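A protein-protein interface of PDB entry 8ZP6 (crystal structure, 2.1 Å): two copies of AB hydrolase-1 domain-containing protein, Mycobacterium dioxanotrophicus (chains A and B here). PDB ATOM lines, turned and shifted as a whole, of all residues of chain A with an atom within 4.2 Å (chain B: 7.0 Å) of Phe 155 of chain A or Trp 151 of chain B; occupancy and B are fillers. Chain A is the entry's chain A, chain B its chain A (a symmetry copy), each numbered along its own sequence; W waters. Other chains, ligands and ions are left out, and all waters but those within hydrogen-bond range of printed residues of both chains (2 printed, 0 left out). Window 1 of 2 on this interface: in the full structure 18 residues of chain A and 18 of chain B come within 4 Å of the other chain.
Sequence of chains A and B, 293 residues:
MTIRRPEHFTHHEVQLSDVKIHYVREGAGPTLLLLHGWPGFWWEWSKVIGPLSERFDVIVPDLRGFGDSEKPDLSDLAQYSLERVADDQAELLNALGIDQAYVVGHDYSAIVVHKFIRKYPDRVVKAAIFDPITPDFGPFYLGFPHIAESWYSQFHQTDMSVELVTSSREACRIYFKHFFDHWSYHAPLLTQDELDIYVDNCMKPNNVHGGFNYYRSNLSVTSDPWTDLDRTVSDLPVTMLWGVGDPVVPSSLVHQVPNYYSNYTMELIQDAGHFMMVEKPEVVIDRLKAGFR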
ATOM      1  N   TRP A 151     -22.167  13.041  -0.043  1.00  0.00           N
ATOM      2  CA  TRP A 151     -20.878  13.729  -0.190  1.00  0.00           C
ATOM      3  C   TRP A 151     -20.106  13.274  -1.439  1.00  0.00           C
ATOM      4  O   TRP A 151     -19.433  14.068  -2.076  1.00  0.00           O
ATOM      5  CB  TRP A 151     -19.997  13.499   1.062  1.00  0.00           C
ATOM      6  CG  TRP A 151     -19.658  12.041   1.229  1.00  0.00           C
ATOM      7  CD1 TRP A 151     -20.355  11.120   1.954  1.00  0.00           C
ATOM      8  CD2 TRP A 151     -18.582  11.324   0.603  1.00  0.00           C
ATOM      9  NE1 TRP A 151     -19.775   9.882   1.830  1.00  0.00           N
ATOM     10  CE2 TRP A 151     -18.687   9.979   1.006  1.00  0.00           C
ATOM     11  CE3 TRP A 151     -17.535  11.692  -0.249  1.00  0.00           C
ATOM     12  CZ2 TRP A 151     -17.792   9.004   0.587  1.00  0.00           C
ATOM     13  CZ3 TRP A 151     -16.663  10.714  -0.689  1.00  0.00           C
ATOM     14  CH2 TRP A 151     -16.795   9.388  -0.265  1.00  0.00           C
ATOM     15  N   TYR A 152     -20.212  11.992  -1.777  1.00  0.00           N
ATOM     16  CA  TYR A 152     -19.428  11.414  -2.868  1.00  0.00           C
ATOM     17  C   TYR A 152     -19.802  12.033  -4.215  1.00  0.00           C
ATOM     18  O   TYR A 152     -18.964  12.121  -5.110  1.00  0.00           O
ATOM     19  CB  TYR A 152     -19.598   9.884  -2.898  1.00  0.00           C
ATOM     20  CG  TYR A 152     -20.988   9.483  -3.288  1.00  0.00           C
ATOM     21  CD1 TYR A 152     -22.023   9.505  -2.358  1.00  0.00           C
ATOM     22  CD2 TYR A 152     -21.279   9.116  -4.584  1.00  0.00           C
ATOM     23  CE1 TYR A 152     -23.305   9.175  -2.722  1.00  0.00           C
ATOM     24  CE2 TYR A 152     -22.556   8.779  -4.952  1.00  0.00           C
ATOM     25  CZ  TYR A 152     -23.563   8.814  -4.018  1.00  0.00           C
ATOM     26  OH  TYR A 152     -24.841   8.489  -4.385  1.00  0.00           O
ATOM     27  N   SER A 153     -21.049  12.483  -4.355  1.00  0.00           N
ATOM     28  CA  SER A 153     -21.490  13.105  -5.603  1.00  0.00           C
ATOM     29  C   SER A 153     -20.715  14.400  -5.852  1.00  0.00           C
ATOM     30  O   SER A 153     -20.531  14.826  -6.995  1.00  0.00           O
ATOM     31  CB  SER A 153     -23.002  13.382  -5.584  1.00  0.00           C
ATOM     32  OG  SER A 153     -23.320  14.439  -4.696  1.00  0.00           O
ATOM     33  N   GLN A 154     -20.252  15.020  -4.775  1.00  0.00           N
ATOM     34  CA  GLN A 154     -19.496  16.261  -4.889  1.00  0.00           C
ATOM     35  C   GLN A 154     -17.984  16.002  -4.980  1.00  0.00           C
ATOM     36  O   GLN A 154     -17.275  16.719  -5.682  1.00  0.00           O
ATOM     37  CB  GLN A 154     -19.833  17.176  -3.713  1.00  0.00           C
ATOM     38  CG  GLN A 154     -21.333  17.452  -3.618  1.00  0.00           C
ATOM     39  CD  GLN A 154     -21.885  18.016  -4.909  1.00  0.00           C
ATOM     40  OE1 GLN A 154     -21.471  19.086  -5.342  1.00  0.00           O
ATOM     41  NE2 GLN A 154     -22.800  17.280  -5.552  1.00  0.00           N
ATOM     42  N   PHE A 155     -17.501  14.981  -4.271  1.00  0.00           N
ATOM     43  CA  PHE A 155     -16.124  14.490  -4.451  1.00  0.00           C
ATOM     44  C   PHE A 155     -15.824  14.235  -5.940  1.00  0.00           C
ATOM     45  O   PHE A 155     -14.767  14.608  -6.463  1.00  0.00           O
ATOM     46  CB  PHE A 155     -15.919  13.206  -3.629  1.00  0.00           C
ATOM     47  CG  PHE A 155     -14.563  12.569  -3.794  1.00  0.00           C
ATOM     48  CD1 PHE A 155     -13.407  13.326  -3.714  1.00  0.00           C
ATOM     49  CD2 PHE A 155     -14.448  11.198  -3.994  1.00  0.00           C
ATOM     50  CE1 PHE A 155     -12.165  12.743  -3.841  1.00  0.00           C
ATOM     51  CE2 PHE A 155     -13.204  10.609  -4.127  1.00  0.00           C
ATOM     52  CZ  PHE A 155     -12.059  11.388  -4.038  1.00  0.00           C
ATOM     53  N   HIS A 156     -16.787  13.624  -6.622  1.00  0.00           N
ATOM     54  CA  HIS A 156     -16.645  13.258  -8.034  1.00  0.00           C
ATOM     55  C   HIS A 156     -16.545  14.448  -8.987  1.00  0.00           C
ATOM     56  O   HIS A 156     -16.192  14.271 -10.149  1.00  0.00           O
ATOM     57  CB  HIS A 156     -17.821  12.373  -8.465  1.00  0.00           C
ATOM     58  CG  HIS A 156     -17.846  11.041  -7.790  1.00  0.00           C
ATOM     59  ND1 HIS A 156     -18.880  10.145  -7.948  1.00  0.00           N
ATOM     60  CD2 HIS A 156     -16.966  10.454  -6.944  1.00  0.00           C
ATOM     61  CE1 HIS A 156     -18.634   9.064  -7.230  1.00  0.00           C
ATOM     62  NE2 HIS A 156     -17.479   9.228  -6.608  1.00  0.00           N
ATOM     63  N   GLN A 157     -16.873  15.645  -8.506  1.00  0.00           N
ATOM     64  CA  GLN A 157     -16.736  16.853  -9.309  1.00  0.00           C
ATOM     65  C   GLN A 157     -15.259  17.212  -9.482  1.00  0.00           C
ATOM     66  O   GLN A 157     -14.911  17.989 -10.364  1.00  0.00           O
ATOM     67  CB  GLN A 157     -17.476  18.048  -8.677  1.00  0.00           C
ATOM     68  CG  GLN A 157     -18.938  17.812  -8.271  1.00  0.00           C
ATOM     69  CD  GLN A 157     -19.863  17.596  -9.454  1.00  0.00           C
ATOM     70  OE1 GLN A 157     -19.668  18.162 -10.526  1.00  0.00           O
ATOM     71  NE2 GLN A 157     -20.872  16.758  -9.263  1.00  0.00           N
ATOM     72  N   THR A 158     -14.390  16.669  -8.635  1.00  0.00           N
ATOM     73  CA  THR A 158     -12.992  17.113  -8.639  1.00  0.00           C
ATOM     74  C   THR A 158     -12.131  16.247  -9.533  1.00  0.00           C
ATOM     75  O   THR A 158     -12.377  15.053  -9.669  1.00  0.00           O
ATOM     76  CB  THR A 158     -12.372  17.108  -7.232  1.00  0.00           C
ATOM     77  OG1 THR A 158     -12.180  15.759  -6.785  1.00  0.00           O
ATOM     78  CG2 THR A 158     -13.250  17.871  -6.241  1.00  0.00           C
ATOM     79  N   MET A 160      -9.191  15.524  -8.738  1.00  0.00           N
ATOM     80  CA  MET A 160      -8.429  14.716  -7.800  1.00  0.00           C
ATOM     81  C   MET A 160      -9.112  13.380  -7.524  1.00  0.00           C
ATOM     82  O   MET A 160      -8.436  12.385  -7.313  1.00  0.00           O
ATOM     83  CB  MET A 160      -8.195  15.472  -6.488  1.00  0.00           C
ATOM     84  CG  MET A 160      -7.403  14.663  -5.455  1.00  0.00           C
ATOM     85  SD  MET A 160      -8.460  13.673  -4.368  1.00  0.00           S
ATOM     86  CE  MET A 160      -9.033  14.967  -3.253  1.00  0.00           C
ATOM     87  N   SER A 161     -10.445  13.348  -7.533  1.00  0.00           N
ATOM     88  CA  SER A 161     -11.131  12.087  -7.300  1.00  0.00           C
ATOM     89  C   SER A 161     -10.735  11.036  -8.343  1.00  0.00           C
ATOM     90  O   SER A 161     -10.467   9.901  -7.986  1.00  0.00           O
ATOM     91  CB  SER A 161     -12.653  12.268  -7.287  1.00  0.00           C
ATOM     92  OG  SER A 161     -13.128  12.767  -8.517  1.00  0.00           O
ATOM     93  N   TYR A 175     -11.855   2.172  -2.474  1.00  0.00           N
ATOM     94  CA  TYR A 175     -12.889   3.173  -2.666  1.00  0.00           C
ATOM     95  C   TYR A 175     -14.246   2.532  -2.920  1.00  0.00           C
ATOM     96  O   TYR A 175     -15.198   2.782  -2.195  1.00  0.00           O
ATOM     97  CB  TYR A 175     -12.522   4.104  -3.820  1.00  0.00           C
ATOM     98  CG  TYR A 175     -13.502   5.238  -3.981  1.00  0.00           C
ATOM     99  CD1 TYR A 175     -13.517   6.289  -3.073  1.00  0.00           C
ATOM    100  CD2 TYR A 175     -14.417   5.257  -5.034  1.00  0.00           C
ATOM    101  CE1 TYR A 175     -14.409   7.330  -3.203  1.00  0.00           C
ATOM    102  CE2 TYR A 175     -15.320   6.296  -5.178  1.00  0.00           C
ATOM    103  CZ  TYR A 175     -15.306   7.334  -4.257  1.00  0.00           C
ATOM    104  OH  TYR A 175     -16.185   8.374  -4.374  1.00  0.00           O
ATOM    105  N   TYR B 141     -22.063  26.185   5.897  1.00  0.00           N
ATOM    106  CA  TYR B 141     -20.999  25.286   5.474  1.00  0.00           C
ATOM    107  C   TYR B 141     -21.523  23.930   4.981  1.00  0.00           C
ATOM    108  O   TYR B 141     -21.070  23.410   3.957  1.00  0.00           O
ATOM    109  CB  TYR B 141     -20.023  25.103   6.634  1.00  0.00           C
ATOM    110  CG  TYR B 141     -18.892  24.126   6.418  1.00  0.00           C
ATOM    111  CD1 TYR B 141     -17.781  24.470   5.654  1.00  0.00           C
ATOM    112  CD2 TYR B 141     -18.911  22.876   7.028  1.00  0.00           C
ATOM    113  CE1 TYR B 141     -16.733  23.597   5.498  1.00  0.00           C
ATOM    114  CE2 TYR B 141     -17.865  21.991   6.869  1.00  0.00           C
ATOM    115  CZ  TYR B 141     -16.783  22.359   6.103  1.00  0.00           C
ATOM    116  OH  TYR B 141     -15.750  21.482   5.943  1.00  0.00           O
ATOM    117  N   LEU B 142     -22.494  23.374   5.693  1.00  0.00           N
ATOM    118  CA  LEU B 142     -23.091  22.105   5.285  1.00  0.00           C
ATOM    119  C   LEU B 142     -24.380  22.336   4.497  1.00  0.00           C
ATOM    120  O   LEU B 142     -25.119  21.402   4.221  1.00  0.00           O
ATOM    121  CB  LEU B 142     -23.360  21.217   6.510  1.00  0.00           C
ATOM    122  CG  LEU B 142     -22.118  20.735   7.275  1.00  0.00           C
ATOM    123  CD1 LEU B 142     -22.494  19.864   8.460  1.00  0.00           C
ATOM    124  CD2 LEU B 142     -21.143  20.004   6.355  1.00  0.00           C
ATOM    125  N   HIS B 146     -22.998  25.082  -0.673  1.00  0.00           N
ATOM    126  CA  HIS B 146     -21.621  24.984  -0.187  1.00  0.00           C
ATOM    127  C   HIS B 146     -21.121  23.543  -0.006  1.00  0.00           C
ATOM    128  O   HIS B 146     -19.913  23.335   0.120  1.00  0.00           O
ATOM    129  CB  HIS B 146     -21.427  25.739   1.125  1.00  0.00           C
ATOM    130  CG  HIS B 146     -20.000  26.133   1.376  1.00  0.00           C
ATOM    131  ND1 HIS B 146     -19.332  27.048   0.590  1.00  0.00           N
ATOM    132  CD2 HIS B 146     -19.103  25.708   2.300  1.00  0.00           C
ATOM    133  CE1 HIS B 146     -18.093  27.188   1.031  1.00  0.00           C
ATOM    134  NE2 HIS B 146     -17.927  26.383   2.063  1.00  0.00           N
ATOM    135  N   ILE B 147     -22.019  22.556  -0.014  1.00  0.00           N
ATOM    136  CA  ILE B 147     -21.581  21.153   0.017  1.00  0.00           C
ATOM    137  C   ILE B 147     -20.662  20.800  -1.151  1.00  0.00           C
ATOM    138  O   ILE B 147     -19.925  19.816  -1.083  1.00  0.00           O
ATOM    139  CB  ILE B 147     -22.754  20.145   0.016  1.00  0.00           C
ATOM    140  CG1 ILE B 147     -23.468  20.099  -1.344  1.00  0.00           C
ATOM    141  CG2 ILE B 147     -23.691  20.434   1.154  1.00  0.00           C
ATOM    142  CD1 ILE B 147     -24.550  21.096  -1.502  1.00  0.00           C
ATOM    143  N   ALA B 148     -20.684  21.600  -2.211  1.00  0.00           N
ATOM    144  CA  ALA B 148     -19.741  21.399  -3.304  1.00  0.00           C
ATOM    145  C   ALA B 148     -18.316  21.598  -2.798  1.00  0.00           C
ATOM    146  O   ALA B 148     -17.378  21.034  -3.341  1.00  0.00           O
ATOM    147  CB  ALA B 148     -20.033  22.344  -4.461  1.00  0.00           C
ATOM    148  N   GLU B 149     -18.172  22.401  -1.746  1.00  0.00           N
ATOM    149  CA  GLU B 149     -16.870  22.664  -1.150  1.00  0.00           C
ATOM    150  C   GLU B 149     -16.640  21.871   0.135  1.00  0.00           C
ATOM    151  O   GLU B 149     -15.502  21.534   0.447  1.00  0.00           O
ATOM    152  CB  GLU B 149     -16.708  24.160  -0.850  1.00  0.00           C
ATOM    153  CG  GLU B 149     -16.780  25.057  -2.065  1.00  0.00           C
ATOM    154  CD  GLU B 149     -15.619  24.844  -3.011  1.00  0.00           C
ATOM    155  OE1 GLU B 149     -15.788  25.094  -4.221  1.00  0.00           O
ATOM    156  OE2 GLU B 149     -14.545  24.411  -2.550  1.00  0.00           O
ATOM    157  N   SER B 150     -17.707  21.590   0.882  1.00  0.00           N
ATOM    158  CA  SER B 150     -17.570  20.975   2.208  1.00  0.00           C
ATOM    159  C   SER B 150     -17.716  19.450   2.248  1.00  0.00           C
ATOM    160  O   SER B 150     -17.671  18.865   3.329  1.00  0.00           O
ATOM    161  CB  SER B 150     -18.585  21.586   3.174  1.00  0.00           C
ATOM    162  OG  SER B 150     -19.914  21.353   2.736  1.00  0.00           O
ATOM    163  N   TRP B 151     -17.884  18.827   1.083  1.00  0.00           N
ATOM    164  CA  TRP B 151     -18.070  17.375   0.955  1.00  0.00           C
ATOM    165  C   TRP B 151     -17.028  16.575   1.753  1.00  0.00           C
ATOM    166  O   TRP B 151     -17.335  15.528   2.299  1.00  0.00           O
ATOM    167  CB  TRP B 151     -18.005  16.951  -0.532  1.00  0.00           C
ATOM    168  CG  TRP B 151     -16.648  17.236  -1.121  1.00  0.00           C
ATOM    169  CD1 TRP B 151     -16.263  18.372  -1.769  1.00  0.00           C
ATOM    170  CD2 TRP B 151     -15.482  16.401  -1.053  1.00  0.00           C
ATOM    171  NE1 TRP B 151     -14.939  18.293  -2.119  1.00  0.00           N
ATOM    172  CE2 TRP B 151     -14.436  17.095  -1.690  1.00  0.00           C
ATOM    173  CE3 TRP B 151     -15.225  15.130  -0.526  1.00  0.00           C
ATOM    174  CZ2 TRP B 151     -13.158  16.566  -1.813  1.00  0.00           C
ATOM    175  CZ3 TRP B 151     -13.945  14.620  -0.622  1.00  0.00           C
ATOM    176  CH2 TRP B 151     -12.929  15.334  -1.266  1.00  0.00           C
ATOM    177  N   TYR B 152     -15.798  17.080   1.811  1.00  0.00           N
ATOM    178  CA  TYR B 152     -14.694  16.351   2.432  1.00  0.00           C
ATOM    179  C   TYR B 152     -14.926  16.151   3.930  1.00  0.00           C
ATOM    180  O   TYR B 152     -14.465  15.165   4.501  1.00  0.00           O
ATOM    181  CB  TYR B 152     -13.360  17.076   2.172  1.00  0.00           C
ATOM    182  CG  TYR B 152     -13.288  18.389   2.890  1.00  0.00           C
ATOM    183  CD1 TYR B 152     -13.917  19.518   2.375  1.00  0.00           C
ATOM    184  CD2 TYR B 152     -12.626  18.499   4.094  1.00  0.00           C
ATOM    185  CE1 TYR B 152     -13.886  20.713   3.049  1.00  0.00           C
ATOM    186  CE2 TYR B 152     -12.586  19.692   4.770  1.00  0.00           C
ATOM    187  CZ  TYR B 152     -13.219  20.792   4.245  1.00  0.00           C
ATOM    188  OH  TYR B 152     -13.191  21.981   4.922  1.00  0.00           O
ATOM    189  N   SER B 153     -15.656  17.070   4.562  1.00  0.00           N
ATOM    190  CA  SER B 153     -15.943  16.952   5.991  1.00  0.00           C
ATOM    191  C   SER B 153     -16.795  15.709   6.260  1.00  0.00           C
ATOM    192  O   SER B 153     -16.753  15.127   7.346  1.00  0.00           O
ATOM    193  CB  SER B 153     -16.649  18.208   6.524  1.00  0.00           C
ATOM    194  OG  SER B 153     -17.981  18.294   6.047  1.00  0.00           O
ATOM    195  N   GLN B 154     -17.561  15.299   5.258  1.00  0.00           N
ATOM    196  CA  GLN B 154     -18.414  14.125   5.396  1.00  0.00           C
ATOM    197  C   GLN B 154     -17.700  12.845   4.933  1.00  0.00           C
ATOM    198  O   GLN B 154     -17.907  11.779   5.509  1.00  0.00           O
ATOM    199  CB  GLN B 154     -19.716  14.345   4.628  1.00  0.00           C
ATOM    200  CG  GLN B 154     -20.441  15.608   5.087  1.00  0.00           C
ATOM    201  CD  GLN B 154     -20.696  15.602   6.579  1.00  0.00           C
ATOM    202  OE1 GLN B 154     -21.393  14.728   7.082  1.00  0.00           O
ATOM    203  NE2 GLN B 154     -20.100  16.559   7.301  1.00  0.00           N
ATOM    204  N   PHE B 155     -16.869  12.956   3.897  1.00  0.00           N
ATOM    205  CA  PHE B 155     -15.959  11.866   3.508  1.00  0.00           C
ATOM    206  C   PHE B 155     -15.160  11.359   4.723  1.00  0.00           C
ATOM    207  O   PHE B 155     -15.011  10.151   4.946  1.00  0.00           O
ATOM    208  CB  PHE B 155     -15.010  12.351   2.399  1.00  0.00           C
ATOM    209  CG  PHE B 155     -13.981  11.337   1.970  1.00  0.00           C
ATOM    210  CD1 PHE B 155     -14.343  10.029   1.691  1.00  0.00           C
ATOM    211  CD2 PHE B 155     -12.650  11.708   1.810  1.00  0.00           C
ATOM    212  CE1 PHE B 155     -13.406   9.107   1.277  1.00  0.00           C
ATOM    213  CE2 PHE B 155     -11.708  10.785   1.399  1.00  0.00           C
ATOM    214  CZ  PHE B 155     -12.094   9.480   1.120  1.00  0.00           C
ATOM    215  N   HIS B 156     -14.678  12.302   5.524  1.00  0.00           N
ATOM    216  CA  HIS B 156     -13.850  11.998   6.695  1.00  0.00           C
ATOM    217  C   HIS B 156     -14.582  11.244   7.806  1.00  0.00           C
ATOM    218  O   HIS B 156     -13.942  10.735   8.720  1.00  0.00           O
ATOM    219  CB  HIS B 156     -13.267  13.292   7.274  1.00  0.00           C
ATOM    220  CG  HIS B 156     -12.296  13.971   6.363  1.00  0.00           C
ATOM    221  ND1 HIS B 156     -11.749  15.203   6.642  1.00  0.00           N
ATOM    222  CD2 HIS B 156     -11.780  13.591   5.170  1.00  0.00           C
ATOM    223  CE1 HIS B 156     -10.936  15.553   5.661  1.00  0.00           C
ATOM    224  NE2 HIS B 156     -10.940  14.592   4.753  1.00  0.00           N
ATOM    225  N   MET B 160     -13.436   4.289   5.441  1.00  0.00           N
ATOM    226  CA  MET B 160     -12.787   4.119   4.151  1.00  0.00           C
ATOM    227  C   MET B 160     -11.880   5.300   3.820  1.00  0.00           C
ATOM    228  O   MET B 160     -10.852   5.116   3.185  1.00  0.00           O
ATOM    229  CB  MET B 160     -13.820   3.916   3.038  1.00  0.00           C
ATOM    230  CG  MET B 160     -13.191   3.742   1.652  1.00  0.00           C
ATOM    231  SD  MET B 160     -12.967   5.309   0.772  1.00  0.00           S
ATOM    232  CE  MET B 160     -14.661   5.582   0.221  1.00  0.00           C
ATOM    233  N   LEU B 164      -8.143   4.651   2.598  1.00  0.00           N
ATOM    234  CA  LEU B 164      -7.747   5.098   1.264  1.00  0.00           C
ATOM    235  C   LEU B 164      -6.572   6.077   1.308  1.00  0.00           C
ATOM    236  O   LEU B 164      -5.581   5.910   0.601  1.00  0.00           O
ATOM    237  CB  LEU B 164      -8.934   5.750   0.544  1.00  0.00           C
ATOM    238  CG  LEU B 164      -8.657   6.322  -0.855  1.00  0.00           C
ATOM    239  CD1 LEU B 164      -8.088   5.233  -1.764  1.00  0.00           C
ATOM    240  CD2 LEU B 164      -9.914   6.900  -1.470  1.00  0.00           C
ATOM    241  N   TYR B 175      -4.262  13.135  -2.444  1.00  0.00           N
ATOM    242  CA  TYR B 175      -5.407  13.642  -1.709  1.00  0.00           C
ATOM    243  C   TYR B 175      -5.154  15.047  -1.180  1.00  0.00           C
ATOM    244  O   TYR B 175      -5.897  15.969  -1.484  1.00  0.00           O
ATOM    245  CB  TYR B 175      -5.761  12.703  -0.558  1.00  0.00           C
ATOM    246  CG  TYR B 175      -7.021  13.117   0.160  1.00  0.00           C
ATOM    247  CD1 TYR B 175      -8.261  12.936  -0.435  1.00  0.00           C
ATOM    248  CD2 TYR B 175      -6.970  13.696   1.428  1.00  0.00           C
ATOM    249  CE1 TYR B 175      -9.420  13.314   0.205  1.00  0.00           C
ATOM    250  CE2 TYR B 175      -8.126  14.082   2.085  1.00  0.00           C
ATOM    251  CZ  TYR B 175      -9.352  13.883   1.465  1.00  0.00           C
ATOM    252  OH  TYR B 175     -10.508  14.252   2.089  1.00  0.00           O
ATOM    253  N   HIS B 178      -4.757  18.401  -3.435  1.00  0.00           N
ATOM    254  CA  HIS B 178      -5.984  19.045  -3.894  1.00  0.00           C
ATOM    255  C   HIS B 178      -6.374  20.210  -2.987  1.00  0.00           C
ATOM    256  O   HIS B 178      -6.724  21.288  -3.458  1.00  0.00           O
ATOM    257  CB  HIS B 178      -7.128  18.030  -3.957  1.00  0.00           C
ATOM    258  CG  HIS B 178      -8.483  18.661  -3.995  1.00  0.00           C
ATOM    259  ND1 HIS B 178      -9.022  19.185  -5.146  1.00  0.00           N
ATOM    260  CD2 HIS B 178      -9.398  18.869  -3.018  1.00  0.00           C
ATOM    261  CE1 HIS B 178     -10.217  19.686  -4.880  1.00  0.00           C
ATOM    262  NE2 HIS B 178     -10.467  19.510  -3.596  1.00  0.00           N
ATOM    263  N   PHE B 179      -6.291  19.999  -1.682  1.00  0.00           N
ATOM    264  CA  PHE B 179      -6.740  21.024  -0.746  1.00  0.00           C
ATOM    265  C   PHE B 179      -5.779  22.202  -0.675  1.00  0.00           C
ATOM    266  O   PHE B 179      -6.224  23.344  -0.674  1.00  0.00           O
ATOM    267  CB  PHE B 179      -6.967  20.403   0.629  1.00  0.00           C
ATOM    268  CG  PHE B 179      -8.046  19.358   0.620  1.00  0.00           C
ATOM    269  CD1 PHE B 179      -9.379  19.724   0.726  1.00  0.00           C
ATOM    270  CD2 PHE B 179      -7.731  18.025   0.448  1.00  0.00           C
ATOM    271  CE1 PHE B 179     -10.378  18.768   0.691  1.00  0.00           C
ATOM    272  CE2 PHE B 179      -8.721  17.058   0.397  1.00  0.00           C
ATOM    273  CZ  PHE B 179     -10.044  17.421   0.525  1.00  0.00           C
ATOM    274  N   HIS B 182      -6.488  23.883  -4.362  1.00  0.00           N
ATOM    275  CA  HIS B 182      -7.837  24.417  -4.593  1.00  0.00           C
ATOM    276  C   HIS B 182      -8.223  25.527  -3.596  1.00  0.00           C
ATOM    277  O   HIS B 182      -8.967  26.444  -3.927  1.00  0.00           O
ATOM    278  CB  HIS B 182      -8.871  23.281  -4.549  1.00  0.00           C
ATOM    279  CG  HIS B 182     -10.293  23.747  -4.618  1.00  0.00           C
ATOM    280  ND1 HIS B 182     -10.779  24.495  -5.666  1.00  0.00           N
ATOM    281  CD2 HIS B 182     -11.335  23.568  -3.768  1.00  0.00           C
ATOM    282  CE1 HIS B 182     -12.060  24.761  -5.461  1.00  0.00           C
ATOM    283  NE2 HIS B 182     -12.419  24.212  -4.313  1.00  0.00           N
HETATM  284  O   HOH W   1      -8.689  18.557  -8.047  1.00  0.00           O
HETATM  285  O   HOH W   2     -17.158  19.613  -5.566  1.00  0.00           O
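Water W2 bridges O of Ala 148 of chain B (2.6 Å) and O of Gln 154 of chain A (2.9 Å). Water W1 lies within hydrogen-bond range of ND1 of His 178 of chain B (3.0 Å) and N of Met 160 of chain A (3.2 Å).
Of the printed residues of chain B, Gln 154 of chain A touches Ile 147, Ala 148 and Trp 151. Phe 155 of chain A touches one residue of chain B. Of chain A, only Trp 151 (3.6 Å), Gln 154 (3.7 Å) and Phe 155 (3.2 Å) come within 4 Å of Trp 151 of chain B. Of the printed residues of chain A, Met 160 of chain B touches Tyr 175. The nearest printed residue of chain A that does not touch Trp 151 of chain B is Met 160 of chain A (4.4 Å).
The side-chain hydroxyl (OG) of Ser 153 of chain A is in hydrogen-bond range of the side-chain amide nitrogen (NE2) of Gln 154 of chain A, 3.0 Å away. O of Phe 155 of chain A sits at hydrogen-bond distance from OG1 of Thr 158 of chain A (2.8 Å). O of Phe 155 of chain A is in hydrogen-bond range of OG of Ser 161 of chain A (3.2 Å). NE2 of His 156 of chain A is in hydrogen-bond range of OH of Tyr 175 of chain A (2.7 Å). O of Thr 158 of chain A lies within hydrogen-bond range of OG of Ser 161 of chain A (2.7 Å). The side-chain hydroxyl (OH) of Tyr 175 of chain B is in hydrogen-bond range of a ring nitrogen (NE2) of His 156 of chain B, 2.7 Å away.
Trp 151 of chain A touches Trp 151 of chain B (CB to O, 3.6 Å). CB of Gln 154 of chain B touches CB of Trp 151 of chain A (3.7 Å). CD1 of Phe 155 of chain B touches CH2 of Trp 151 of chain A (3.2 Å). CB of Gln 154 of chain A touches O of Ile 147 of chain B, 3.7 Å away. Gln 154 of chain A touches Ala 148 of chain B. Gln 154 of chain A touches Trp 151 of chain B. CE of Met 160 of chain A touches CD1 of Tyr 175 of chain B, at 3.6 Å. Met 160 of chain A touches His 178 of chain B. Met 160 of chain B touches Tyr 175 of chain A. CD1 of Tyr 175 of chain A touches CD2 of Leu 164 of chain B, 3.99 Å away.
Hydrophobic or aromatic side chains of chain A that line the printed part of chain B: Trp 151, Phe 155, Met 160 and Tyr 175. Among the printed residues, 12 pairs touch across the chains. Among the printed residues, no Asp or Glu carboxylate lies within 4 Å of a Lys or Arg side-chain nitrogen of the other chain.
Trp 151 of chain A touches its own counterpart, Trp 151 of chain B. Trp 151 of chain A touches Gln 154 of chain B, and with the chains exchanged Gln 154 of chain A touches Trp 151 of chain B. Trp 151 of chain A touches Phe 155 of chain B, and with the chains exchanged Phe 155 of chain A touches Trp 151 of chain B. Met 160 of chain A touches Tyr 175 of chain B, and with the chains exchanged Tyr 175 of chain A touches Met 160 of chain B. Positions printed for both chains: 151, 152, 153, 154, 155, 156, 160 and 175. Of the 12 pairs that touch across the chains among the printed residues, 7 have their exchanged pair printed and touching as well.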
